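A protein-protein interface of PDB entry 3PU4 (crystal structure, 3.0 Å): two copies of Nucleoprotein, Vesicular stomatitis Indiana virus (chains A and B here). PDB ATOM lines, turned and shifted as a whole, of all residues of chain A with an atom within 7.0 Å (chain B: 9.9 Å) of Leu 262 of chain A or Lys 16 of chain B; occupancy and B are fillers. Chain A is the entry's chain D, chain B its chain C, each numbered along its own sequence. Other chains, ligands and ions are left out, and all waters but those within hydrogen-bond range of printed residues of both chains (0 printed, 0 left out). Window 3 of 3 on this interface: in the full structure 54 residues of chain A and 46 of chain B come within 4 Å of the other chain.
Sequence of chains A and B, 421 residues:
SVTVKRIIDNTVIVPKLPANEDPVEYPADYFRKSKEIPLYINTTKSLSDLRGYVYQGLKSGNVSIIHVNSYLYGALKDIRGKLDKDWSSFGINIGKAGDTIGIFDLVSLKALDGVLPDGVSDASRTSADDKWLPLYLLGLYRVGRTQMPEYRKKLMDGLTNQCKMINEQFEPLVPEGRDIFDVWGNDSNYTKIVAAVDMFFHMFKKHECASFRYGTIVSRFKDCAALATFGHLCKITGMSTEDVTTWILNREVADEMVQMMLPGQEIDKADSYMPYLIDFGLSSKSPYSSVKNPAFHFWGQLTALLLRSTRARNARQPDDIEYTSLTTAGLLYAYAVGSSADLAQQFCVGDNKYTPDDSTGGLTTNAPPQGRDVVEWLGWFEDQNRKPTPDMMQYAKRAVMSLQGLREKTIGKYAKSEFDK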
ATOM      1  N   TYR A  26       6.677 -17.088 -12.683  1.00  0.00           N
ATOM      2  CA  TYR A  26       7.034 -18.487 -12.458  1.00  0.00           C
ATOM      3  C   TYR A  26       6.809 -19.291 -13.724  1.00  0.00           C
ATOM      4  O   TYR A  26       6.096 -18.845 -14.625  1.00  0.00           O
ATOM      5  CB  TYR A  26       6.205 -19.087 -11.335  1.00  0.00           C
ATOM      6  CG  TYR A  26       6.487 -18.508  -9.970  1.00  0.00           C
ATOM      7  CD1 TYR A  26       5.874 -17.337  -9.550  1.00  0.00           C
ATOM      8  CD2 TYR A  26       7.352 -19.141  -9.092  1.00  0.00           C
ATOM      9  CE1 TYR A  26       6.132 -16.793  -8.295  1.00  0.00           C
ATOM     10  CE2 TYR A  26       7.616 -18.613  -7.837  1.00  0.00           C
ATOM     11  CZ  TYR A  26       7.006 -17.434  -7.440  1.00  0.00           C
ATOM     12  OH  TYR A  26       7.258 -16.910  -6.180  1.00  0.00           O
ATOM     13  N   ASP A  29       2.903 -21.038 -13.980  1.00  0.00           N
ATOM     14  CA  ASP A  29       1.960 -19.966 -14.322  1.00  0.00           C
ATOM     15  C   ASP A  29       2.385 -19.397 -15.712  1.00  0.00           C
ATOM     16  O   ASP A  29       2.641 -18.196 -15.850  1.00  0.00           O
ATOM     17  CB  ASP A  29       1.877 -18.842 -13.217  1.00  0.00           C
ATOM     18  CG  ASP A  29       1.545 -19.390 -11.731  1.00  0.00           C
ATOM     19  OD1 ASP A  29       1.534 -20.616 -11.443  1.00  0.00           O
ATOM     20  OD2 ASP A  29       1.305 -18.566 -10.807  1.00  0.00           O
ATOM     21  N   LEU A 227      18.625 -20.269  -5.628  1.00  0.00           N
ATOM     22  CA  LEU A 227      18.496 -21.700  -5.454  1.00  0.00           C
ATOM     23  C   LEU A 227      19.847 -22.326  -5.224  1.00  0.00           C
ATOM     24  O   LEU A 227      20.010 -23.146  -4.354  1.00  0.00           O
ATOM     25  CB  LEU A 227      17.861 -22.348  -6.674  1.00  0.00           C
ATOM     26  CG  LEU A 227      16.359 -22.217  -6.694  1.00  0.00           C
ATOM     27  CD1 LEU A 227      15.811 -23.035  -7.805  1.00  0.00           C
ATOM     28  CD2 LEU A 227      15.883 -22.724  -5.380  1.00  0.00           C
ATOM     29  N   PHE A 230      21.408 -21.623  -1.864  1.00  0.00           N
ATOM     30  CA  PHE A 230      20.706 -22.363  -0.808  1.00  0.00           C
ATOM     31  C   PHE A 230      21.212 -23.798  -0.740  1.00  0.00           C
ATOM     32  O   PHE A 230      21.459 -24.337   0.335  1.00  0.00           O
ATOM     33  CB  PHE A 230      19.217 -22.361  -1.095  1.00  0.00           C
ATOM     34  CG  PHE A 230      18.403 -23.132  -0.119  1.00  0.00           C
ATOM     35  CD1 PHE A 230      18.619 -23.007   1.245  1.00  0.00           C
ATOM     36  CD2 PHE A 230      17.370 -23.939  -0.557  1.00  0.00           C
ATOM     37  CE1 PHE A 230      17.844 -23.695   2.158  1.00  0.00           C
ATOM     38  CE2 PHE A 230      16.588 -24.622   0.342  1.00  0.00           C
ATOM     39  CZ  PHE A 230      16.831 -24.508   1.709  1.00  0.00           C
ATOM     40  N   THR A 241      17.736 -29.522   4.714  1.00  0.00           N
ATOM     41  CA  THR A 241      17.126 -28.356   4.098  1.00  0.00           C
ATOM     42  C   THR A 241      16.104 -27.714   5.046  1.00  0.00           C
ATOM     43  O   THR A 241      15.954 -26.486   5.087  1.00  0.00           O
ATOM     44  CB  THR A 241      16.491 -28.698   2.753  1.00  0.00           C
ATOM     45  OG1 THR A 241      15.126 -29.084   2.944  1.00  0.00           O
ATOM     46  CG2 THR A 241      17.243 -29.851   2.116  1.00  0.00           C
ATOM     47  N   GLU A 242      15.412 -28.528   5.831  1.00  0.00           N
ATOM     48  CA  GLU A 242      14.391 -27.950   6.686  1.00  0.00           C
ATOM     49  C   GLU A 242      15.023 -27.312   7.897  1.00  0.00           C
ATOM     50  O   GLU A 242      14.510 -26.326   8.396  1.00  0.00           O
ATOM     51  CB  GLU A 242      13.327 -28.961   7.076  1.00  0.00           C
ATOM     52  CG  GLU A 242      13.840 -30.382   7.066  1.00  0.00           C
ATOM     53  CD  GLU A 242      13.717 -31.044   5.705  1.00  0.00           C
ATOM     54  OE1 GLU A 242      12.621 -30.960   5.106  1.00  0.00           O
ATOM     55  OE2 GLU A 242      14.708 -31.656   5.239  1.00  0.00           O
ATOM     56  N   THR A 245      16.442 -23.916   6.913  1.00  0.00           N
ATOM     57  CA  THR A 245      15.362 -22.947   6.804  1.00  0.00           C
ATOM     58  C   THR A 245      15.072 -22.275   8.124  1.00  0.00           C
ATOM     59  O   THR A 245      14.815 -21.080   8.158  1.00  0.00           O
ATOM     60  CB  THR A 245      14.053 -23.581   6.360  1.00  0.00           C
ATOM     61  OG1 THR A 245      14.193 -24.112   5.044  1.00  0.00           O
ATOM     62  CG2 THR A 245      12.970 -22.541   6.348  1.00  0.00           C
ATOM     63  N   MET A 257      12.669 -16.377   0.791  1.00  0.00           N
ATOM     64  CA  MET A 257      12.645 -17.823   0.805  1.00  0.00           C
ATOM     65  C   MET A 257      11.295 -18.331   0.387  1.00  0.00           C
ATOM     66  O   MET A 257      11.210 -19.166  -0.481  1.00  0.00           O
ATOM     67  CB  MET A 257      12.953 -18.357   2.187  1.00  0.00           C
ATOM     68  CG  MET A 257      12.830 -19.852   2.259  1.00  0.00           C
ATOM     69  SD  MET A 257      14.193 -20.545   1.338  1.00  0.00           S
ATOM     70  CE  MET A 257      14.076 -22.275   1.797  1.00  0.00           C
ATOM     71  N   VAL A 258      10.237 -17.840   1.023  1.00  0.00           N
ATOM     72  CA  VAL A 258       8.879 -18.277   0.699  1.00  0.00           C
ATOM     73  C   VAL A 258       8.647 -18.138  -0.799  1.00  0.00           C
ATOM     74  O   VAL A 258       8.090 -19.024  -1.428  1.00  0.00           O
ATOM     75  CB  VAL A 258       7.806 -17.456   1.430  1.00  0.00           C
ATOM     76  CG1 VAL A 258       6.462 -17.708   0.804  1.00  0.00           C
ATOM     77  CG2 VAL A 258       7.780 -17.786   2.894  1.00  0.00           C
ATOM     78  N   GLN A 259       9.098 -17.032  -1.370  1.00  0.00           N
ATOM     79  CA  GLN A 259       8.955 -16.809  -2.796  1.00  0.00           C
ATOM     80  C   GLN A 259       9.627 -17.916  -3.608  1.00  0.00           C
ATOM     81  O   GLN A 259       9.116 -18.317  -4.648  1.00  0.00           O
ATOM     82  CB  GLN A 259       9.502 -15.425  -3.176  1.00  0.00           C
ATOM     83  CG  GLN A 259      10.138 -15.334  -4.575  1.00  0.00           C
ATOM     84  CD  GLN A 259      10.838 -14.000  -4.832  1.00  0.00           C
ATOM     85  OE1 GLN A 259      10.184 -12.969  -4.966  1.00  0.00           O
ATOM     86  NE2 GLN A 259      12.171 -14.018  -4.901  1.00  0.00           N
ATOM     87  N   MET A 260      10.758 -18.419  -3.131  1.00  0.00           N
ATOM     88  CA  MET A 260      11.536 -19.365  -3.913  1.00  0.00           C
ATOM     89  C   MET A 260      10.955 -20.767  -3.853  1.00  0.00           C
ATOM     90  O   MET A 260      11.107 -21.554  -4.777  1.00  0.00           O
ATOM     91  CB  MET A 260      12.987 -19.399  -3.445  1.00  0.00           C
ATOM     92  CG  MET A 260      13.661 -18.058  -3.429  1.00  0.00           C
ATOM     93  SD  MET A 260      15.413 -18.354  -3.330  1.00  0.00           S
ATOM     94  CE  MET A 260      15.689 -18.629  -1.593  1.00  0.00           C
ATOM     95  N   MET A 261      10.280 -21.087  -2.767  1.00  0.00           N
ATOM     96  CA  MET A 261       9.823 -22.445  -2.558  1.00  0.00           C
ATOM     97  C   MET A 261       8.348 -22.598  -2.913  1.00  0.00           C
ATOM     98  O   MET A 261       7.707 -23.574  -2.554  1.00  0.00           O
ATOM     99  CB  MET A 261      10.070 -22.862  -1.113  1.00  0.00           C
ATOM    100  CG  MET A 261      11.503 -22.788  -0.663  1.00  0.00           C
ATOM    101  SD  MET A 261      12.517 -24.025  -1.446  1.00  0.00           S
ATOM    102  CE  MET A 261      12.978 -23.231  -3.008  1.00  0.00           C
ATOM    103  N   LEU A 262       7.806 -21.624  -3.624  1.00  0.00           N
ATOM    104  CA  LEU A 262       6.457 -21.756  -4.156  1.00  0.00           C
ATOM    105  C   LEU A 262       6.301 -23.111  -4.826  1.00  0.00           C
ATOM    106  O   LEU A 262       7.170 -23.542  -5.580  1.00  0.00           O
ATOM    107  CB  LEU A 262       6.184 -20.687  -5.199  1.00  0.00           C
ATOM    108  CG  LEU A 262       4.690 -20.547  -5.435  1.00  0.00           C
ATOM    109  CD1 LEU A 262       4.105 -19.973  -4.155  1.00  0.00           C
ATOM    110  CD2 LEU A 262       4.408 -19.668  -6.651  1.00  0.00           C
ATOM    111  N   PRO A 263       5.180 -23.784  -4.559  1.00  0.00           N
ATOM    112  CA  PRO A 263       4.975 -25.176  -4.968  1.00  0.00           C
ATOM    113  C   PRO A 263       4.523 -25.353  -6.412  1.00  0.00           C
ATOM    114  O   PRO A 263       4.058 -24.422  -7.074  1.00  0.00           O
ATOM    115  CB  PRO A 263       3.877 -25.675  -4.016  1.00  0.00           C
ATOM    116  CG  PRO A 263       3.740 -24.604  -2.956  1.00  0.00           C
ATOM    117  CD  PRO A 263       4.138 -23.332  -3.628  1.00  0.00           C
ATOM    118  N   GLY A 264       4.675 -26.585  -6.885  1.00  0.00           N
ATOM    119  CA  GLY A 264       4.284 -26.946  -8.228  1.00  0.00           C
ATOM    120  C   GLY A 264       5.057 -26.214  -9.292  1.00  0.00           C
ATOM    121  O   GLY A 264       4.493 -25.859 -10.324  1.00  0.00           O
ATOM    122  N   GLN A 265       6.347 -25.999  -9.051  1.00  0.00           N
ATOM    123  CA  GLN A 265       7.212 -25.383 -10.047  1.00  0.00           C
ATOM    124  C   GLN A 265       8.290 -26.344 -10.518  1.00  0.00           C
ATOM    125  O   GLN A 265       9.132 -25.991 -11.326  1.00  0.00           O
ATOM    126  CB  GLN A 265       7.844 -24.139  -9.465  1.00  0.00           C
ATOM    127  CG  GLN A 265       6.824 -23.173  -8.932  1.00  0.00           C
ATOM    128  CD  GLN A 265       5.930 -22.606 -10.026  1.00  0.00           C
ATOM    129  OE1 GLN A 265       4.716 -22.421  -9.814  1.00  0.00           O
ATOM    130  NE2 GLN A 265       6.519 -22.327 -11.209  1.00  0.00           N
ATOM    131  N   GLU A 266       8.269 -27.557  -9.983  1.00  0.00           N
ATOM    132  CA  GLU A 266       9.126 -28.623 -10.477  1.00  0.00           C
ATOM    133  C   GLU A 266      10.620 -28.426 -10.231  1.00  0.00           C
ATOM    134  O   GLU A 266      11.430 -29.032 -10.925  1.00  0.00           O
ATOM    135  CB  GLU A 266       8.868 -28.848 -11.967  1.00  0.00           C
ATOM    136  CG  GLU A 266       7.968 -30.040 -12.257  1.00  0.00           C
ATOM    137  CD  GLU A 266       7.410 -30.033 -13.670  1.00  0.00           C
ATOM    138  OE1 GLU A 266       7.374 -31.117 -14.317  1.00  0.00           O
ATOM    139  OE2 GLU A 266       7.013 -28.936 -14.127  1.00  0.00           O
ATOM    140  N   ILE A 267      10.997 -27.613  -9.243  1.00  0.00           N
ATOM    141  CA  ILE A 267      12.424 -27.369  -9.020  1.00  0.00           C
ATOM    142  C   ILE A 267      13.205 -28.582  -8.516  1.00  0.00           C
ATOM    143  O   ILE A 267      14.384 -28.737  -8.835  1.00  0.00           O
ATOM    144  CB  ILE A 267      12.696 -26.138  -8.150  1.00  0.00           C
ATOM    145  CG1 ILE A 267      12.366 -26.393  -6.696  1.00  0.00           C
ATOM    146  CG2 ILE A 267      11.870 -24.980  -8.622  1.00  0.00           C
ATOM    147  CD1 ILE A 267      12.251 -25.095  -5.893  1.00  0.00           C
ATOM    148  N   ASP A 268      12.548 -29.456  -7.762  1.00  0.00           N
ATOM    149  CA  ASP A 268      13.208 -30.659  -7.268  1.00  0.00           C
ATOM    150  C   ASP A 268      13.082 -31.831  -8.234  1.00  0.00           C
ATOM    151  O   ASP A 268      13.549 -32.941  -7.931  1.00  0.00           O
ATOM    152  CB  ASP A 268      12.679 -31.056  -5.888  1.00  0.00           C
ATOM    153  CG  ASP A 268      11.173 -31.335  -5.872  1.00  0.00           C
ATOM    154  OD1 ASP A 268      10.623 -31.588  -4.762  1.00  0.00           O
ATOM    155  OD2 ASP A 268      10.546 -31.298  -6.961  1.00  0.00           O
ATOM    156  N   TYR A 288      13.950 -16.936  -8.925  1.00  0.00           N
ATOM    157  CA  TYR A 288      15.059 -17.541  -8.213  1.00  0.00           C
ATOM    158  C   TYR A 288      16.366 -16.759  -8.381  1.00  0.00           C
ATOM    159  O   TYR A 288      17.427 -17.171  -7.913  1.00  0.00           O
ATOM    160  CB  TYR A 288      15.220 -18.954  -8.753  1.00  0.00           C
ATOM    161  CG  TYR A 288      13.889 -19.648  -8.904  1.00  0.00           C
ATOM    162  CD1 TYR A 288      13.251 -20.170  -7.804  1.00  0.00           C
ATOM    163  CD2 TYR A 288      13.263 -19.762 -10.134  1.00  0.00           C
ATOM    164  CE1 TYR A 288      12.040 -20.799  -7.918  1.00  0.00           C
ATOM    165  CE2 TYR A 288      12.043 -20.389 -10.258  1.00  0.00           C
ATOM    166  CZ  TYR A 288      11.433 -20.908  -9.141  1.00  0.00           C
ATOM    167  OH  TYR A 288      10.216 -21.551  -9.209  1.00  0.00           O
ATOM    168  N   VAL B   2       9.680 -33.007   8.860  1.00  0.00           N
ATOM    169  CA  VAL B   2       8.953 -33.021   7.599  1.00  0.00           C
ATOM    170  C   VAL B   2       8.093 -31.755   7.449  1.00  0.00           C
ATOM    171  O   VAL B   2       7.648 -31.432   6.352  1.00  0.00           O
ATOM    172  CB  VAL B   2       8.081 -34.309   7.438  1.00  0.00           C
ATOM    173  CG1 VAL B   2       7.811 -34.611   5.951  1.00  0.00           C
ATOM    174  CG2 VAL B   2       8.748 -35.511   8.113  1.00  0.00           C
ATOM    175  N   VAL B   4       7.523 -27.490   8.278  1.00  0.00           N
ATOM    176  CA  VAL B   4       8.038 -26.191   8.681  1.00  0.00           C
ATOM    177  C   VAL B   4       6.959 -25.117   8.569  1.00  0.00           C
ATOM    178  O   VAL B   4       6.383 -24.947   7.504  1.00  0.00           O
ATOM    179  CB  VAL B   4       9.161 -25.765   7.736  1.00  0.00           C
ATOM    180  CG1 VAL B   4       9.688 -24.389   8.130  1.00  0.00           C
ATOM    181  CG2 VAL B   4      10.266 -26.812   7.696  1.00  0.00           C
ATOM    182  N   VAL B  12       2.423 -22.926   6.031  1.00  0.00           N
ATOM    183  CA  VAL B  12       3.464 -23.906   5.771  1.00  0.00           C
ATOM    184  C   VAL B  12       4.315 -23.547   4.554  1.00  0.00           C
ATOM    185  O   VAL B  12       3.798 -23.168   3.497  1.00  0.00           O
ATOM    186  CB  VAL B  12       2.876 -25.288   5.508  1.00  0.00           C
ATOM    187  CG1 VAL B  12       3.016 -26.156   6.727  1.00  0.00           C
ATOM    188  CG2 VAL B  12       1.425 -25.159   5.070  1.00  0.00           C
ATOM    189  N   ILE B  13       5.627 -23.679   4.722  1.00  0.00           N
ATOM    190  CA  ILE B  13       6.584 -23.556   3.635  1.00  0.00           C
ATOM    191  C   ILE B  13       7.208 -24.942   3.465  1.00  0.00           C
ATOM    192  O   ILE B  13       7.420 -25.658   4.439  1.00  0.00           O
ATOM    193  CB  ILE B  13       7.651 -22.476   3.944  1.00  0.00           C
ATOM    194  CG1 ILE B  13       8.457 -22.130   2.703  1.00  0.00           C
ATOM    195  CG2 ILE B  13       8.597 -22.918   5.023  1.00  0.00           C
ATOM    196  CD1 ILE B  13       9.406 -20.936   2.913  1.00  0.00           C
ATOM    197  N   VAL B  14       7.468 -25.352   2.231  1.00  0.00           N
ATOM    198  CA  VAL B  14       8.033 -26.683   2.007  1.00  0.00           C
ATOM    199  C   VAL B  14       9.383 -26.640   1.327  1.00  0.00           C
ATOM    200  O   VAL B  14       9.465 -26.723   0.087  1.00  0.00           O
ATOM    201  CB  VAL B  14       7.132 -27.527   1.117  1.00  0.00           C
ATOM    202  CG1 VAL B  14       7.561 -28.981   1.167  1.00  0.00           C
ATOM    203  CG2 VAL B  14       5.692 -27.360   1.545  1.00  0.00           C
ATOM    204  N   PRO B  15      10.450 -26.535   2.136  1.00  0.00           N
ATOM    205  CA  PRO B  15      11.802 -26.350   1.607  1.00  0.00           C
ATOM    206  C   PRO B  15      12.149 -27.508   0.712  1.00  0.00           C
ATOM    207  O   PRO B  15      12.118 -28.652   1.147  1.00  0.00           O
ATOM    208  CB  PRO B  15      12.679 -26.386   2.858  1.00  0.00           C
ATOM    209  CG  PRO B  15      11.786 -25.949   3.924  1.00  0.00           C
ATOM    210  CD  PRO B  15      10.449 -26.557   3.599  1.00  0.00           C
ATOM    211  N   LYS B  16      12.467 -27.204  -0.531  1.00  0.00           N
ATOM    212  CA  LYS B  16      12.946 -28.209  -1.435  1.00  0.00           C
ATOM    213  C   LYS B  16      14.055 -27.565  -2.258  1.00  0.00           C
ATOM    214  O   LYS B  16      14.131 -26.338  -2.345  1.00  0.00           O
ATOM    215  CB  LYS B  16      11.795 -28.663  -2.319  1.00  0.00           C
ATOM    216  CG  LYS B  16      10.735 -27.585  -2.486  1.00  0.00           C
ATOM    217  CD  LYS B  16       9.769 -27.871  -3.640  1.00  0.00           C
ATOM    218  CE  LYS B  16       8.849 -26.664  -3.868  1.00  0.00           C
ATOM    219  NZ  LYS B  16       8.236 -26.167  -2.581  1.00  0.00           N
ATOM    220  N   LEU B  17      14.923 -28.383  -2.849  1.00  0.00           N
ATOM    221  CA  LEU B  17      15.962 -27.856  -3.745  1.00  0.00           C
ATOM    222  C   LEU B  17      16.326 -28.824  -4.866  1.00  0.00           C
ATOM    223  O   LEU B  17      16.163 -30.029  -4.726  1.00  0.00           O
ATOM    224  CB  LEU B  17      17.195 -27.381  -2.959  1.00  0.00           C
ATOM    225  CG  LEU B  17      18.268 -28.324  -2.438  1.00  0.00           C
ATOM    226  CD1 LEU B  17      19.078 -27.554  -1.428  1.00  0.00           C
ATOM    227  CD2 LEU B  17      17.679 -29.564  -1.816  1.00  0.00           C
ATOM    228  N   PRO B  18      16.805 -28.285  -5.997  1.00  0.00           N
ATOM    229  CA  PRO B  18      17.072 -29.016  -7.244  1.00  0.00           C
ATOM    230  C   PRO B  18      17.625 -30.423  -7.077  1.00  0.00           C
ATOM    231  O   PRO B  18      18.498 -30.672  -6.263  1.00  0.00           O
ATOM    232  CB  PRO B  18      18.101 -28.132  -7.931  1.00  0.00           C
ATOM    233  CG  PRO B  18      17.680 -26.762  -7.551  1.00  0.00           C
ATOM    234  CD  PRO B  18      17.133 -26.856  -6.138  1.00  0.00           C
ATOM    235  N   ALA B  19      17.114 -31.336  -7.889  1.00  0.00           N
ATOM    236  CA  ALA B  19      17.533 -32.730  -7.844  1.00  0.00           C
ATOM    237  C   ALA B  19      18.903 -32.890  -8.471  1.00  0.00           C
ATOM    238  O   ALA B  19      19.181 -32.319  -9.520  1.00  0.00           O
ATOM    239  CB  ALA B  19      16.519 -33.619  -8.566  1.00  0.00           C
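The side-chain amino group (NZ) of Lys 16 of chain B lies within hydrogen-bond range of the backbone carbonyl oxygen (O) of Met 261 of chain A, 2.6 Å away.
The backbone carbonyl oxygen (O) of Val 4 of chain B sits at hydrogen-bond distance from the backbone NH (N) of Ile 13 of chain B (3.1 Å).
O of Val 14 of chain B lies within hydrogen-bond range of NZ of Lys 16 of chain B (3.0 Å).
The side-chain hydroxyl of Thr 241 of chain A sits at hydrogen-bond distance from the side-chain carboxylate of Glu 242 of chain A (3.5 Å).
OG1 of Thr 245 of chain A is in hydrogen-bond range of O of Thr 241 of chain A.
Leu 17 of chain B touches Thr 241 of chain A (CD2 to CG2, 3.97 Å).
Val 4 of chain B touches Glu 242 of chain A (CG2 to CB, 3.8 Å).
Pro 15 of chain B touches Thr 245 of chain A (CG to OG1, 3.2 Å).
CA of Val 258 of chain A touches CD1 of Ile 13 of chain B, at 3.5 Å.
Pro 15 of chain B touches Met 261 of chain A.
Leu 262 of chain A touches Lys 16 of chain B (O to CE, 3.9 Å).
Pro 18 of chain B touches Ile 267 of chain A.
Lys 16 of chain B touches Asp 268 of chain A.
CB of Asp 268 of chain A touches O of Leu 17 of chain B, at 3.8 Å.
CB of Ala 19 of chain B touches O of Asp 268 of chain A (3.1 Å).
Of chain B, only Pro 15 and Lys 16 come within 4 Å of Met 261 of chain A.
Of the printed residues of chain B, Leu 262 of chain A touches Lys 16 (3.9 Å).
No residue of chain B comes within 4 Å of Pro 263 of chain A.
Of the printed residues of chain B, Ile 267 of chain A touches Pro 18 (3.1 Å) and Ala 19 (3.9 Å).
Printed residues of chain A within 4 Å of Val 4 of chain B: Glu 242.
Lys 16 of chain B touches three residues of chain A.
The nearest residue of chain B that does not touch Leu 262 of chain A is Ile 13 of chain B (6.4 Å).
The nearest residue of chain A that does not touch Lys 16 of chain B is Phe 230 of chain A (4.03 Å).
Hydrophobic or aromatic side chains of chain B that line the printed part of chain A: Val 4, Ile 13, Pro 15, Leu 17, Pro 18 and Ala 19.
Of the 20 printed residues of chain A, 9 touch a printed residue of chain B.
Among the printed residues, 14 pairs touch across the chains.
No position is printed for both chains.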
